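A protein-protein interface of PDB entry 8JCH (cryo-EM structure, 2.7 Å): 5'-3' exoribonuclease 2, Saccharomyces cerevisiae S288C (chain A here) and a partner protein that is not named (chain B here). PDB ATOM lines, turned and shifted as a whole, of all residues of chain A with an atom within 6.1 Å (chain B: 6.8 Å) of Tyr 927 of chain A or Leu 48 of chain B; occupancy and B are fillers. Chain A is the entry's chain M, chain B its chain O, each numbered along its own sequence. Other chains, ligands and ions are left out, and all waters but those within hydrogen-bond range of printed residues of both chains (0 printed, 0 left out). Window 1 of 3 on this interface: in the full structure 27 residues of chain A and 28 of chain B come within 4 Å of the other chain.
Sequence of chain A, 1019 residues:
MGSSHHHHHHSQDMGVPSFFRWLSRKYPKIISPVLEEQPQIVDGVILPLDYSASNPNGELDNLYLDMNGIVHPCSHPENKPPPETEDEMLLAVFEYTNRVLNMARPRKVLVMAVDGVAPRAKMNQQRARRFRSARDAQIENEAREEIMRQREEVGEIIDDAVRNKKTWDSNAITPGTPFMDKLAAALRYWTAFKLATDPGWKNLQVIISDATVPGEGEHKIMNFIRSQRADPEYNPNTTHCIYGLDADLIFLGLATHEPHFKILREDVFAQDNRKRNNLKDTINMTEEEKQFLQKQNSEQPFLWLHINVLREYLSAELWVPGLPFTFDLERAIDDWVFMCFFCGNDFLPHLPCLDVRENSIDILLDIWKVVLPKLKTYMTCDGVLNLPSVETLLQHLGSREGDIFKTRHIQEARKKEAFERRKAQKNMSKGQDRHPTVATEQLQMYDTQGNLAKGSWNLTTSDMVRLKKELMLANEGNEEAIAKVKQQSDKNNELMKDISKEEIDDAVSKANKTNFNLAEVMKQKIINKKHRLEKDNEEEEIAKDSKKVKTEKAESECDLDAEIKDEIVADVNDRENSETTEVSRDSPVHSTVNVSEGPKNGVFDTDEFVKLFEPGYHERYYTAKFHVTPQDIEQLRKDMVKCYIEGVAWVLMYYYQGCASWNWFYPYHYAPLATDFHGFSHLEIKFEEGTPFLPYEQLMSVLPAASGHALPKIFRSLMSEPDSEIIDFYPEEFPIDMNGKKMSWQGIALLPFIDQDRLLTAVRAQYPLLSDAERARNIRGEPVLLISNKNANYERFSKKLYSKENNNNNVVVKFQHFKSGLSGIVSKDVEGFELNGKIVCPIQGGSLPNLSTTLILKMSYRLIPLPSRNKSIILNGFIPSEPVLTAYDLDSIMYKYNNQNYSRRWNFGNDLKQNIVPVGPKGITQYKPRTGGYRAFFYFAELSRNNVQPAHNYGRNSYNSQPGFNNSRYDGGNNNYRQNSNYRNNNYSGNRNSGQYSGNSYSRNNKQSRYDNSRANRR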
ATOM      1  N   ASN A 876      22.766 -24.682  -1.397  1.00  0.00           N
ATOM      2  CA  ASN A 876      22.094 -24.029  -0.283  1.00  0.00           C
ATOM      3  C   ASN A 876      21.822 -22.562  -0.600  1.00  0.00           C
ATOM      4  O   ASN A 876      22.600 -21.894  -1.286  1.00  0.00           O
ATOM      5  CB  ASN A 876      22.937 -24.141   0.988  1.00  0.00           C
ATOM      6  CG  ASN A 876      22.144 -23.827   2.241  1.00  0.00           C
ATOM      7  OD1 ASN A 876      20.917 -23.755   2.211  1.00  0.00           O
ATOM      8  ND2 ASN A 876      22.847 -23.637   3.352  1.00  0.00           N
ATOM      9  N   PHE A 878      19.248 -21.515  -2.378  1.00  0.00           N
ATOM     10  CA  PHE A 878      18.527 -21.360  -3.633  1.00  0.00           C
ATOM     11  C   PHE A 878      17.092 -20.921  -3.366  1.00  0.00           C
ATOM     12  O   PHE A 878      16.403 -21.495  -2.517  1.00  0.00           O
ATOM     13  CB  PHE A 878      18.549 -22.673  -4.416  1.00  0.00           C
ATOM     14  CG  PHE A 878      17.421 -22.817  -5.396  1.00  0.00           C
ATOM     15  CD1 PHE A 878      17.399 -22.068  -6.561  1.00  0.00           C
ATOM     16  CD2 PHE A 878      16.386 -23.704  -5.156  1.00  0.00           C
ATOM     17  CE1 PHE A 878      16.364 -22.202  -7.466  1.00  0.00           C
ATOM     18  CE2 PHE A 878      15.348 -23.841  -6.057  1.00  0.00           C
ATOM     19  CZ  PHE A 878      15.337 -23.088  -7.213  1.00  0.00           C
ATOM     20  N   PRO A 880      13.385 -20.870  -4.397  1.00  0.00           N
ATOM     21  CA  PRO A 880      12.515 -21.644  -5.290  1.00  0.00           C
ATOM     22  C   PRO A 880      11.738 -20.739  -6.235  1.00  0.00           C
ATOM     23  O   PRO A 880      11.363 -19.617  -5.887  1.00  0.00           O
ATOM     24  CB  PRO A 880      11.581 -22.385  -4.325  1.00  0.00           C
ATOM     25  CG  PRO A 880      12.273 -22.343  -2.996  1.00  0.00           C
ATOM     26  CD  PRO A 880      13.036 -21.058  -2.980  1.00  0.00           C
ATOM     27  N   THR A 925      13.435 -15.196   1.649  1.00  0.00           N
ATOM     28  CA  THR A 925      13.322 -16.520   2.245  1.00  0.00           C
ATOM     29  C   THR A 925      13.419 -17.596   1.171  1.00  0.00           C
ATOM     30  O   THR A 925      12.799 -17.489   0.109  1.00  0.00           O
ATOM     31  CB  THR A 925      12.000 -16.649   3.002  1.00  0.00           C
ATOM     32  OG1 THR A 925      11.802 -15.490   3.823  1.00  0.00           O
ATOM     33  CG2 THR A 925      12.006 -17.891   3.882  1.00  0.00           C
ATOM     34  N   GLN A 926      14.201 -18.636   1.450  1.00  0.00           N
ATOM     35  CA  GLN A 926      14.393 -19.740   0.519  1.00  0.00           C
ATOM     36  C   GLN A 926      13.437 -20.899   0.766  1.00  0.00           C
ATOM     37  O   GLN A 926      13.541 -21.924   0.084  1.00  0.00           O
ATOM     38  CB  GLN A 926      15.838 -20.245   0.590  1.00  0.00           C
ATOM     39  CG  GLN A 926      16.261 -20.726   1.968  1.00  0.00           C
ATOM     40  CD  GLN A 926      17.342 -21.788   1.906  1.00  0.00           C
ATOM     41  OE1 GLN A 926      17.600 -22.367   0.852  1.00  0.00           O
ATOM     42  NE2 GLN A 926      17.980 -22.048   3.041  1.00  0.00           N
ATOM     43  N   TYR A 927      12.520 -20.770   1.720  1.00  0.00           N
ATOM     44  CA  TYR A 927      11.557 -21.815   2.039  1.00  0.00           C
ATOM     45  C   TYR A 927      10.146 -21.273   1.866  1.00  0.00           C
ATOM     46  O   TYR A 927       9.810 -20.221   2.420  1.00  0.00           O
ATOM     47  CB  TYR A 927      11.757 -22.332   3.467  1.00  0.00           C
ATOM     48  CG  TYR A 927      13.134 -22.897   3.727  1.00  0.00           C
ATOM     49  CD1 TYR A 927      13.562 -24.055   3.091  1.00  0.00           C
ATOM     50  CD2 TYR A 927      14.008 -22.273   4.607  1.00  0.00           C
ATOM     51  CE1 TYR A 927      14.820 -24.576   3.325  1.00  0.00           C
ATOM     52  CE2 TYR A 927      15.268 -22.786   4.848  1.00  0.00           C
ATOM     53  CZ  TYR A 927      15.668 -23.937   4.205  1.00  0.00           C
ATOM     54  OH  TYR A 927      16.922 -24.452   4.441  1.00  0.00           O
ATOM     55  N   LYS A 928       9.329 -21.989   1.099  1.00  0.00           N
ATOM     56  CA  LYS A 928       7.944 -21.593   0.918  1.00  0.00           C
ATOM     57  C   LYS A 928       7.164 -21.815   2.214  1.00  0.00           C
ATOM     58  O   LYS A 928       7.542 -22.652   3.039  1.00  0.00           O
ATOM     59  CB  LYS A 928       7.307 -22.381  -0.225  1.00  0.00           C
ATOM     60  CG  LYS A 928       7.042 -23.843   0.085  1.00  0.00           C
ATOM     61  CD  LYS A 928       6.005 -24.426  -0.861  1.00  0.00           C
ATOM     62  CE  LYS A 928       5.596 -25.828  -0.441  1.00  0.00           C
ATOM     63  NZ  LYS A 928       5.932 -26.839  -1.481  1.00  0.00           N
ATOM     64  N   PRO A 929       6.084 -21.063   2.429  1.00  0.00           N
ATOM     65  CA  PRO A 929       5.312 -21.223   3.668  1.00  0.00           C
ATOM     66  C   PRO A 929       4.728 -22.624   3.788  1.00  0.00           C
ATOM     67  O   PRO A 929       4.051 -23.116   2.882  1.00  0.00           O
ATOM     68  CB  PRO A 929       4.214 -20.159   3.545  1.00  0.00           C
ATOM     69  CG  PRO A 929       4.159 -19.818   2.090  1.00  0.00           C
ATOM     70  CD  PRO A 929       5.558 -19.973   1.591  1.00  0.00           C
ATOM     71  N   ARG A 930       5.000 -23.263   4.922  1.00  0.00           N
ATOM     72  CA  ARG A 930       4.524 -24.607   5.239  1.00  0.00           C
ATOM     73  C   ARG A 930       3.923 -24.628   6.638  1.00  0.00           C
ATOM     74  O   ARG A 930       4.252 -25.473   7.473  1.00  0.00           O
ATOM     75  CB  ARG A 930       5.648 -25.631   5.114  1.00  0.00           C
ATOM     76  CG  ARG A 930       7.042 -25.045   5.252  1.00  0.00           C
ATOM     77  CD  ARG A 930       8.109 -26.098   5.001  1.00  0.00           C
ATOM     78  NE  ARG A 930       8.010 -26.674   3.666  1.00  0.00           N
ATOM     79  CZ  ARG A 930       8.442 -26.083   2.559  1.00  0.00           C
ATOM     80  NH1 ARG A 930       9.015 -24.891   2.590  1.00  0.00           N
ATOM     81  NH2 ARG A 930       8.297 -26.705   1.393  1.00  0.00           N
ATOM     82  N   TYR B  46      25.673 -25.034   7.080  1.00  0.00           N
ATOM     83  CA  TYR B  46      24.240 -25.277   6.990  1.00  0.00           C
ATOM     84  C   TYR B  46      23.881 -25.904   5.648  1.00  0.00           C
ATOM     85  O   TYR B  46      24.386 -25.498   4.597  1.00  0.00           O
ATOM     86  CB  TYR B  46      23.469 -23.971   7.181  1.00  0.00           C
ATOM     87  CG  TYR B  46      21.979 -24.155   7.362  1.00  0.00           C
ATOM     88  CD1 TYR B  46      21.430 -24.339   8.624  1.00  0.00           C
ATOM     89  CD2 TYR B  46      21.119 -24.141   6.271  1.00  0.00           C
ATOM     90  CE1 TYR B  46      20.069 -24.507   8.794  1.00  0.00           C
ATOM     91  CE2 TYR B  46      19.757 -24.308   6.431  1.00  0.00           C
ATOM     92  CZ  TYR B  46      19.237 -24.490   7.695  1.00  0.00           C
ATOM     93  OH  TYR B  46      17.881 -24.657   7.859  1.00  0.00           O
ATOM     94  N   TYR B  47      23.000 -26.902   5.691  1.00  0.00           N
ATOM     95  CA  TYR B  47      22.526 -27.558   4.475  1.00  0.00           C
ATOM     96  C   TYR B  47      21.180 -28.200   4.781  1.00  0.00           C
ATOM     97  O   TYR B  47      21.124 -29.192   5.514  1.00  0.00           O
ATOM     98  CB  TYR B  47      23.533 -28.591   3.984  1.00  0.00           C
ATOM     99  CG  TYR B  47      22.986 -29.521   2.926  1.00  0.00           C
ATOM    100  CD1 TYR B  47      22.557 -29.031   1.700  1.00  0.00           C
ATOM    101  CD2 TYR B  47      22.902 -30.888   3.151  1.00  0.00           C
ATOM    102  CE1 TYR B  47      22.058 -29.877   0.728  1.00  0.00           C
ATOM    103  CE2 TYR B  47      22.404 -31.742   2.185  1.00  0.00           C
ATOM    104  CZ  TYR B  47      21.984 -31.230   0.976  1.00  0.00           C
ATOM    105  OH  TYR B  47      21.487 -32.076   0.011  1.00  0.00           O
ATOM    106  N   LEU B  48      20.109 -27.640   4.222  1.00  0.00           N
ATOM    107  CA  LEU B  48      18.759 -28.151   4.459  1.00  0.00           C
ATOM    108  C   LEU B  48      17.904 -27.863   3.238  1.00  0.00           C
ATOM    109  O   LEU B  48      17.320 -26.778   3.107  1.00  0.00           O
ATOM    110  CB  LEU B  48      18.136 -27.539   5.712  1.00  0.00           C
ATOM    111  CG  LEU B  48      17.190 -28.432   6.521  1.00  0.00           C
ATOM    112  CD1 LEU B  48      15.758 -28.289   6.025  1.00  0.00           C
ATOM    113  CD2 LEU B  48      17.636 -29.887   6.473  1.00  0.00           C
ATOM    114  N   PRO B  49      17.811 -28.812   2.310  1.00  0.00           N
ATOM    115  CA  PRO B  49      16.955 -28.620   1.136  1.00  0.00           C
ATOM    116  C   PRO B  49      15.482 -28.587   1.518  1.00  0.00           C
ATOM    117  O   PRO B  49      15.062 -29.119   2.548  1.00  0.00           O
ATOM    118  CB  PRO B  49      17.270 -29.833   0.253  1.00  0.00           C
ATOM    119  CG  PRO B  49      18.542 -30.409   0.803  1.00  0.00           C
ATOM    120  CD  PRO B  49      18.536 -30.091   2.261  1.00  0.00           C
ATOM    121  N   ASP B  50      14.694 -27.935   0.659  1.00  0.00           N
ATOM    122  CA  ASP B  50      13.256 -27.846   0.896  1.00  0.00           C
ATOM    123  C   ASP B  50      12.594 -29.217   0.864  1.00  0.00           C
ATOM    124  O   ASP B  50      11.535 -29.409   1.474  1.00  0.00           O
ATOM    125  CB  ASP B  50      12.612 -26.921  -0.138  1.00  0.00           C
ATOM    126  CG  ASP B  50      11.722 -25.872   0.496  1.00  0.00           C
ATOM    127  OD1 ASP B  50      11.431 -25.989   1.706  1.00  0.00           O
ATOM    128  OD2 ASP B  50      11.313 -24.929  -0.212  1.00  0.00           O
ATOM    129  N   ALA B  51      13.195 -30.179   0.158  1.00  0.00           N
ATOM    130  CA  ALA B  51      12.655 -31.534   0.146  1.00  0.00           C
ATOM    131  C   ALA B  51      12.698 -32.155   1.536  1.00  0.00           C
ATOM    132  O   ALA B  51      11.762 -32.855   1.942  1.00  0.00           O
ATOM    133  CB  ALA B  51      13.423 -32.398  -0.854  1.00  0.00           C
ATOM    134  N   GLU B  52      13.780 -31.914   2.280  1.00  0.00           N
ATOM    135  CA  GLU B  52      13.862 -32.409   3.650  1.00  0.00           C
ATOM    136  C   GLU B  52      12.789 -31.780   4.529  1.00  0.00           C
ATOM    137  O   GLU B  52      12.188 -32.458   5.370  1.00  0.00           O
ATOM    138  CB  GLU B  52      15.253 -32.141   4.223  1.00  0.00           C
ATOM    139  CG  GLU B  52      16.139 -33.374   4.307  1.00  0.00           C
ATOM    140  CD  GLU B  52      16.811 -33.701   2.987  1.00  0.00           C
ATOM    141  OE1 GLU B  52      16.724 -32.878   2.053  1.00  0.00           O
ATOM    142  OE2 GLU B  52      17.424 -34.785   2.885  1.00  0.00           O
ATOM    143  N   LEU B  53      12.539 -30.480   4.352  1.00  0.00           N
ATOM    144  CA  LEU B  53      11.479 -29.819   5.107  1.00  0.00           C
ATOM    145  C   LEU B  53      10.115 -30.408   4.770  1.00  0.00           C
ATOM    146  O   LEU B  53       9.277 -30.604   5.659  1.00  0.00           O
ATOM    147  CB  LEU B  53      11.496 -28.316   4.831  1.00  0.00           C
ATOM    148  CG  LEU B  53      12.012 -27.420   5.957  1.00  0.00           C
ATOM    149  CD1 LEU B  53      11.796 -25.957   5.608  1.00  0.00           C
ATOM    150  CD2 LEU B  53      11.335 -27.767   7.274  1.00  0.00           C
ATOM    151  N   LEU B  57      10.441 -35.534   8.712  1.00  0.00           N
ATOM    152  CA  LEU B  57      11.637 -35.906   9.453  1.00  0.00           C
ATOM    153  C   LEU B  57      11.322 -36.072  10.935  1.00  0.00           C
ATOM    154  O   LEU B  57      10.504 -35.341  11.501  1.00  0.00           O
ATOM    155  CB  LEU B  57      12.730 -34.853   9.264  1.00  0.00           C
ATOM    156  CG  LEU B  57      13.816 -35.144   8.225  1.00  0.00           C
ATOM    157  CD1 LEU B  57      14.887 -36.051   8.809  1.00  0.00           C
ATOM    158  CD2 LEU B  57      13.225 -35.752   6.961  1.00  0.00           C
ATOM    159  N   PHE B 171      18.146 -31.499  15.863  1.00  0.00           N
ATOM    160  CA  PHE B 171      17.899 -30.499  14.830  1.00  0.00           C
ATOM    161  C   PHE B 171      19.199 -29.843  14.391  1.00  0.00           C
ATOM    162  O   PHE B 171      19.406 -29.592  13.199  1.00  0.00           O
ATOM    163  CB  PHE B 171      16.907 -29.452  15.335  1.00  0.00           C
ATOM    164  CG  PHE B 171      16.780 -28.256  14.435  1.00  0.00           C
ATOM    165  CD1 PHE B 171      16.295 -28.394  13.145  1.00  0.00           C
ATOM    166  CD2 PHE B 171      17.145 -26.996  14.877  1.00  0.00           C
ATOM    167  CE1 PHE B 171      16.176 -27.296  12.313  1.00  0.00           C
ATOM    168  CE2 PHE B 171      17.028 -25.894  14.050  1.00  0.00           C
ATOM    169  CZ  PHE B 171      16.543 -26.045  12.766  1.00  0.00           C
ATOM    170  N   LEU B 174      21.135 -32.554  12.079  1.00  0.00           N
ATOM    171  CA  LEU B 174      20.639 -32.588  10.704  1.00  0.00           C
ATOM    172  C   LEU B 174      20.604 -31.218  10.036  1.00  0.00           C
ATOM    173  O   LEU B 174      20.325 -31.146   8.835  1.00  0.00           O
ATOM    174  CB  LEU B 174      19.248 -33.234  10.601  1.00  0.00           C
ATOM    175  CG  LEU B 174      19.009 -34.686  11.034  1.00  0.00           C
ATOM    176  CD1 LEU B 174      20.194 -35.560  10.652  1.00  0.00           C
ATOM    177  CD2 LEU B 174      18.659 -34.854  12.490  1.00  0.00           C
ATOM    178  N   ALA B 175      20.874 -30.140  10.767  1.00  0.00           N
ATOM    179  CA  ALA B 175      20.960 -28.812  10.177  1.00  0.00           C
ATOM    180  C   ALA B 175      22.392 -28.363   9.921  1.00  0.00           C
ATOM    181  O   ALA B 175      22.604 -27.210   9.535  1.00  0.00           O
ATOM    182  CB  ALA B 175      20.252 -27.791  11.073  1.00  0.00           C
ATOM    183  N   ARG B 192      24.884 -38.875   7.388  1.00  0.00           N
ATOM    184  CA  ARG B 192      24.499 -37.774   8.264  1.00  0.00           C
ATOM    185  C   ARG B 192      22.992 -37.743   8.483  1.00  0.00           C
ATOM    186  O   ARG B 192      22.524 -37.400   9.575  1.00  0.00           O
ATOM    187  CB  ARG B 192      24.983 -36.447   7.680  1.00  0.00           C
ATOM    188  CG  ARG B 192      25.280 -35.374   8.718  1.00  0.00           C
ATOM    189  CD  ARG B 192      24.054 -34.517   8.998  1.00  0.00           C
ATOM    190  NE  ARG B 192      23.178 -34.412   7.838  1.00  0.00           N
ATOM    191  CZ  ARG B 192      23.120 -33.358   7.036  1.00  0.00           C
ATOM    192  NH1 ARG B 192      23.880 -32.293   7.236  1.00  0.00           N
ATOM    193  NH2 ARG B 192      22.279 -33.371   6.005  1.00  0.00           N
ATOM    194  N   PHE B 226      26.057 -20.665   6.935  1.00  0.00           N
ATOM    195  CA  PHE B 226      25.051 -20.810   5.887  1.00  0.00           C
ATOM    196  C   PHE B 226      25.643 -20.536   4.510  1.00  0.00           C
ATOM    197  O   PHE B 226      25.446 -21.317   3.571  1.00  0.00           O
ATOM    198  CB  PHE B 226      23.874 -19.875   6.165  1.00  0.00           C
ATOM    199  CG  PHE B 226      22.784 -19.948   5.133  1.00  0.00           C
ATOM    200  CD1 PHE B 226      21.852 -20.971   5.164  1.00  0.00           C
ATOM    201  CD2 PHE B 226      22.688 -18.991   4.137  1.00  0.00           C
ATOM    202  CE1 PHE B 226      20.847 -21.040   4.218  1.00  0.00           C
ATOM    203  CE2 PHE B 226      21.686 -19.055   3.188  1.00  0.00           C
ATOM    204  CZ  PHE B 226      20.764 -20.081   3.229  1.00  0.00           C
ATOM    205  N   ILE B 277      18.070 -18.001  11.838  1.00  0.00           N
ATOM    206  CA  ILE B 277      17.184 -19.088  11.440  1.00  0.00           C
ATOM    207  C   ILE B 277      16.663 -19.833  12.663  1.00  0.00           C
ATOM    208  O   ILE B 277      17.414 -20.151  13.590  1.00  0.00           O
ATOM    209  CB  ILE B 277      17.924 -20.038  10.480  1.00  0.00           C
ATOM    210  CG1 ILE B 277      18.207 -19.338   9.149  1.00  0.00           C
ATOM    211  CG2 ILE B 277      17.131 -21.316  10.260  1.00  0.00           C
ATOM    212  CD1 ILE B 277      19.274 -20.016   8.317  1.00  0.00           C
ATOM    213  N   LEU B 287       9.701 -31.820  12.473  1.00  0.00           N
ATOM    214  CA  LEU B 287      10.034 -30.530  11.887  1.00  0.00           C
ATOM    215  C   LEU B 287       8.960 -30.109  10.891  1.00  0.00           C
ATOM    216  O   LEU B 287       8.537 -30.901  10.044  1.00  0.00           O
ATOM    217  CB  LEU B 287      11.398 -30.599  11.201  1.00  0.00           C
ATOM    218  CG  LEU B 287      12.022 -29.265  10.784  1.00  0.00           C
ATOM    219  CD1 LEU B 287      12.121 -28.321  11.972  1.00  0.00           C
ATOM    220  CD2 LEU B 287      13.389 -29.486  10.155  1.00  0.00           C
ATOM    221  N   THR B 289       8.500 -26.155   9.814  1.00  0.00           N
ATOM    222  CA  THR B 289       8.872 -24.976   9.045  1.00  0.00           C
ATOM    223  C   THR B 289      10.218 -24.449   9.519  1.00  0.00           C
ATOM    224  O   THR B 289      10.520 -24.476  10.715  1.00  0.00           O
ATOM    225  CB  THR B 289       7.812 -23.871   9.167  1.00  0.00           C
ATOM    226  OG1 THR B 289       6.504 -24.447   9.059  1.00  0.00           O
ATOM    227  CG2 THR B 289       7.992 -22.830   8.071  1.00  0.00           C
ATOM    228  N   VAL B 290      11.023 -23.973   8.571  1.00  0.00           N
ATOM    229  CA  VAL B 290      12.298 -23.326   8.850  1.00  0.00           C
ATOM    230  C   VAL B 290      12.269 -21.944   8.214  1.00  0.00           C
ATOM    231  O   VAL B 290      11.954 -21.809   7.026  1.00  0.00           O
ATOM    232  CB  VAL B 290      13.484 -24.153   8.320  1.00  0.00           C
ATOM    233  CG1 VAL B 290      14.763 -23.334   8.353  1.00  0.00           C
ATOM    234  CG2 VAL B 290      13.642 -25.430   9.129  1.00  0.00           C
ATOM    235  N   GLU B 291      12.591 -20.922   9.001  1.00  0.00           N
ATOM    236  CA  GLU B 291      12.500 -19.539   8.559  1.00  0.00           C
ATOM    237  C   GLU B 291      13.886 -18.967   8.262  1.00  0.00           C
ATOM    238  O   GLU B 291      14.916 -19.606   8.483  1.00  0.00           O
ATOM    239  CB  GLU B 291      11.776 -18.694   9.613  1.00  0.00           C
ATOM    240  CG  GLU B 291      12.393 -18.762  10.998  1.00  0.00           C
ATOM    241  CD  GLU B 291      13.439 -17.692  11.205  1.00  0.00           C
ATOM    242  OE1 GLU B 291      13.621 -16.873  10.285  1.00  0.00           O
ATOM    243  OE2 GLU B 291      14.076 -17.664  12.277  1.00  0.00           O
ATOM    244  N   GLU B 292      13.893 -17.738   7.748  1.00  0.00           N
ATOM    245  CA  GLU B 292      15.112 -17.073   7.287  1.00  0.00           C
ATOM    246  C   GLU B 292      15.154 -15.621   7.766  1.00  0.00           C
ATOM    247  O   GLU B 292      15.354 -14.692   6.981  1.00  0.00           O
ATOM    248  CB  GLU B 292      15.229 -17.145   5.765  1.00  0.00           C
ATOM    249  CG  GLU B 292      15.384 -18.554   5.212  1.00  0.00           C
ATOM    250  CD  GLU B 292      16.710 -19.186   5.590  1.00  0.00           C
ATOM    251  OE1 GLU B 292      17.763 -18.623   5.227  1.00  0.00           O
ATOM    252  OE2 GLU B 292      16.697 -20.247   6.248  1.00  0.00           O
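Tyr 927 of chain A touches just these residues of chain B: Tyr 46 (3.5 Å), Leu 48 (2.7 Å), Asp 50 (3.2 Å), Leu 53 (3.6 Å), Val 290 (3.2 Å) and Glu 292 (3.2 Å). Leu 48 of chain B touches just one residue of chain A: Tyr 927. Printed residues of chain B within 4 Å of Thr 925 of chain A: Glu 292. Printed residues of chain B within 4 Å of Arg 930 of chain A: Asp 50, Leu 53 and Thr 289. Printed residues of chain A within 4 Å of Asp 50 of chain B: Pro 880 (3.9 Å), Gln 926 (3.8 Å), Tyr 927 (3.2 Å), Lys 928 (3.8 Å) and Arg 930 (2.8 Å). Printed residues of chain A within 4 Å of Tyr 46 of chain B: Asn 876 and Tyr 927. Of the printed residues of chain A, Leu 53 of chain B touches Tyr 927 (3.6 Å) and Arg 930 (3.7 Å). Pro 929 of chain A touches none of the printed residues of chain B. Tyr 47 of chain B touches none of the printed residues of chain A. The nearest residue of chain B that does not touch Tyr 927 of chain A is Pro 49 of chain B (4.4 Å). The nearest residue of chain A that does not touch Leu 48 of chain B is Asn 876 of chain A (4.4 Å).
Of the 20 printed residues of chain B, 8 touch a printed residue of chain A. Hydrophobic or aromatic side chains of chain B that line the printed part of chain A: Tyr 46, Leu 48, Leu 53, Phe 226 and Val 290. Of the 9 printed residues of chain A, 7 touch a printed residue of chain B.
OD1 of Asn 876 of chain A is in hydrogen-bond range of NE2 of Gln 926 of chain A (3.5 Å). O of Lys 928 of chain A lies within hydrogen-bond range of NH1 of Arg 930 of chain A (2.7 Å). The side-chain amide nitrogen of Gln 926 of chain A lies within hydrogen-bond range of the side-chain hydroxyl of Tyr 927 of chain A, at 3.0 Å.
Among the printed residues, pairs that only touch across the chains: Tyr 927 of chain A with Asp 50 of chain B (3.2 Å), Tyr 927 of chain A with Val 290 of chain B (3.2 Å), Tyr 927 of chain A with Glu 292 of chain B (3.2 Å), Gln 926 of chain A with Phe 226 of chain B (3.3 Å), Tyr 927 of chain A with Tyr 46 of chain B (3.5 Å), Tyr 927 of chain A with Leu 53 of chain B (3.6 Å), Thr 925 of chain A with Glu 292 of chain B (3.7 Å), Arg 930 of chain A with Leu 53 of chain B (3.7 Å), Gln 926 of chain A with Asp 50 of chain B (3.8 Å), Lys 928 of chain A with Asp 50 of chain B (3.8 Å), Gln 926 of chain A with Glu 292 of chain B (3.9 Å) and Pro 880 of chain A with Asp 50 of chain B (3.9 Å).
O of Arg 930 of chain A lies within hydrogen-bond range of OG1 of Thr 289 of chain B (2.9 Å). NH1 of Arg 930 of chain A is in salt-bridge range of OD1 of Asp 50 of chain B (2.8 Å). The side-chain hydroxyl (OH) of Tyr 927 of chain A sits at hydrogen-bond distance from the backbone carbonyl oxygen (O) of Leu 48 of chain B (2.7 Å). The side-chain amide nitrogen (ND2) of Asn 876 of chain A lies within hydrogen-bond range of the backbone carbonyl oxygen (O) of Tyr 46 of chain B (2.7 Å). The side-chain amide nitrogen (ND2) of Asn 876 of chain A sits close to the backbone carbonyl oxygen (O) of Phe 226 of chain B (3.5 Å).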
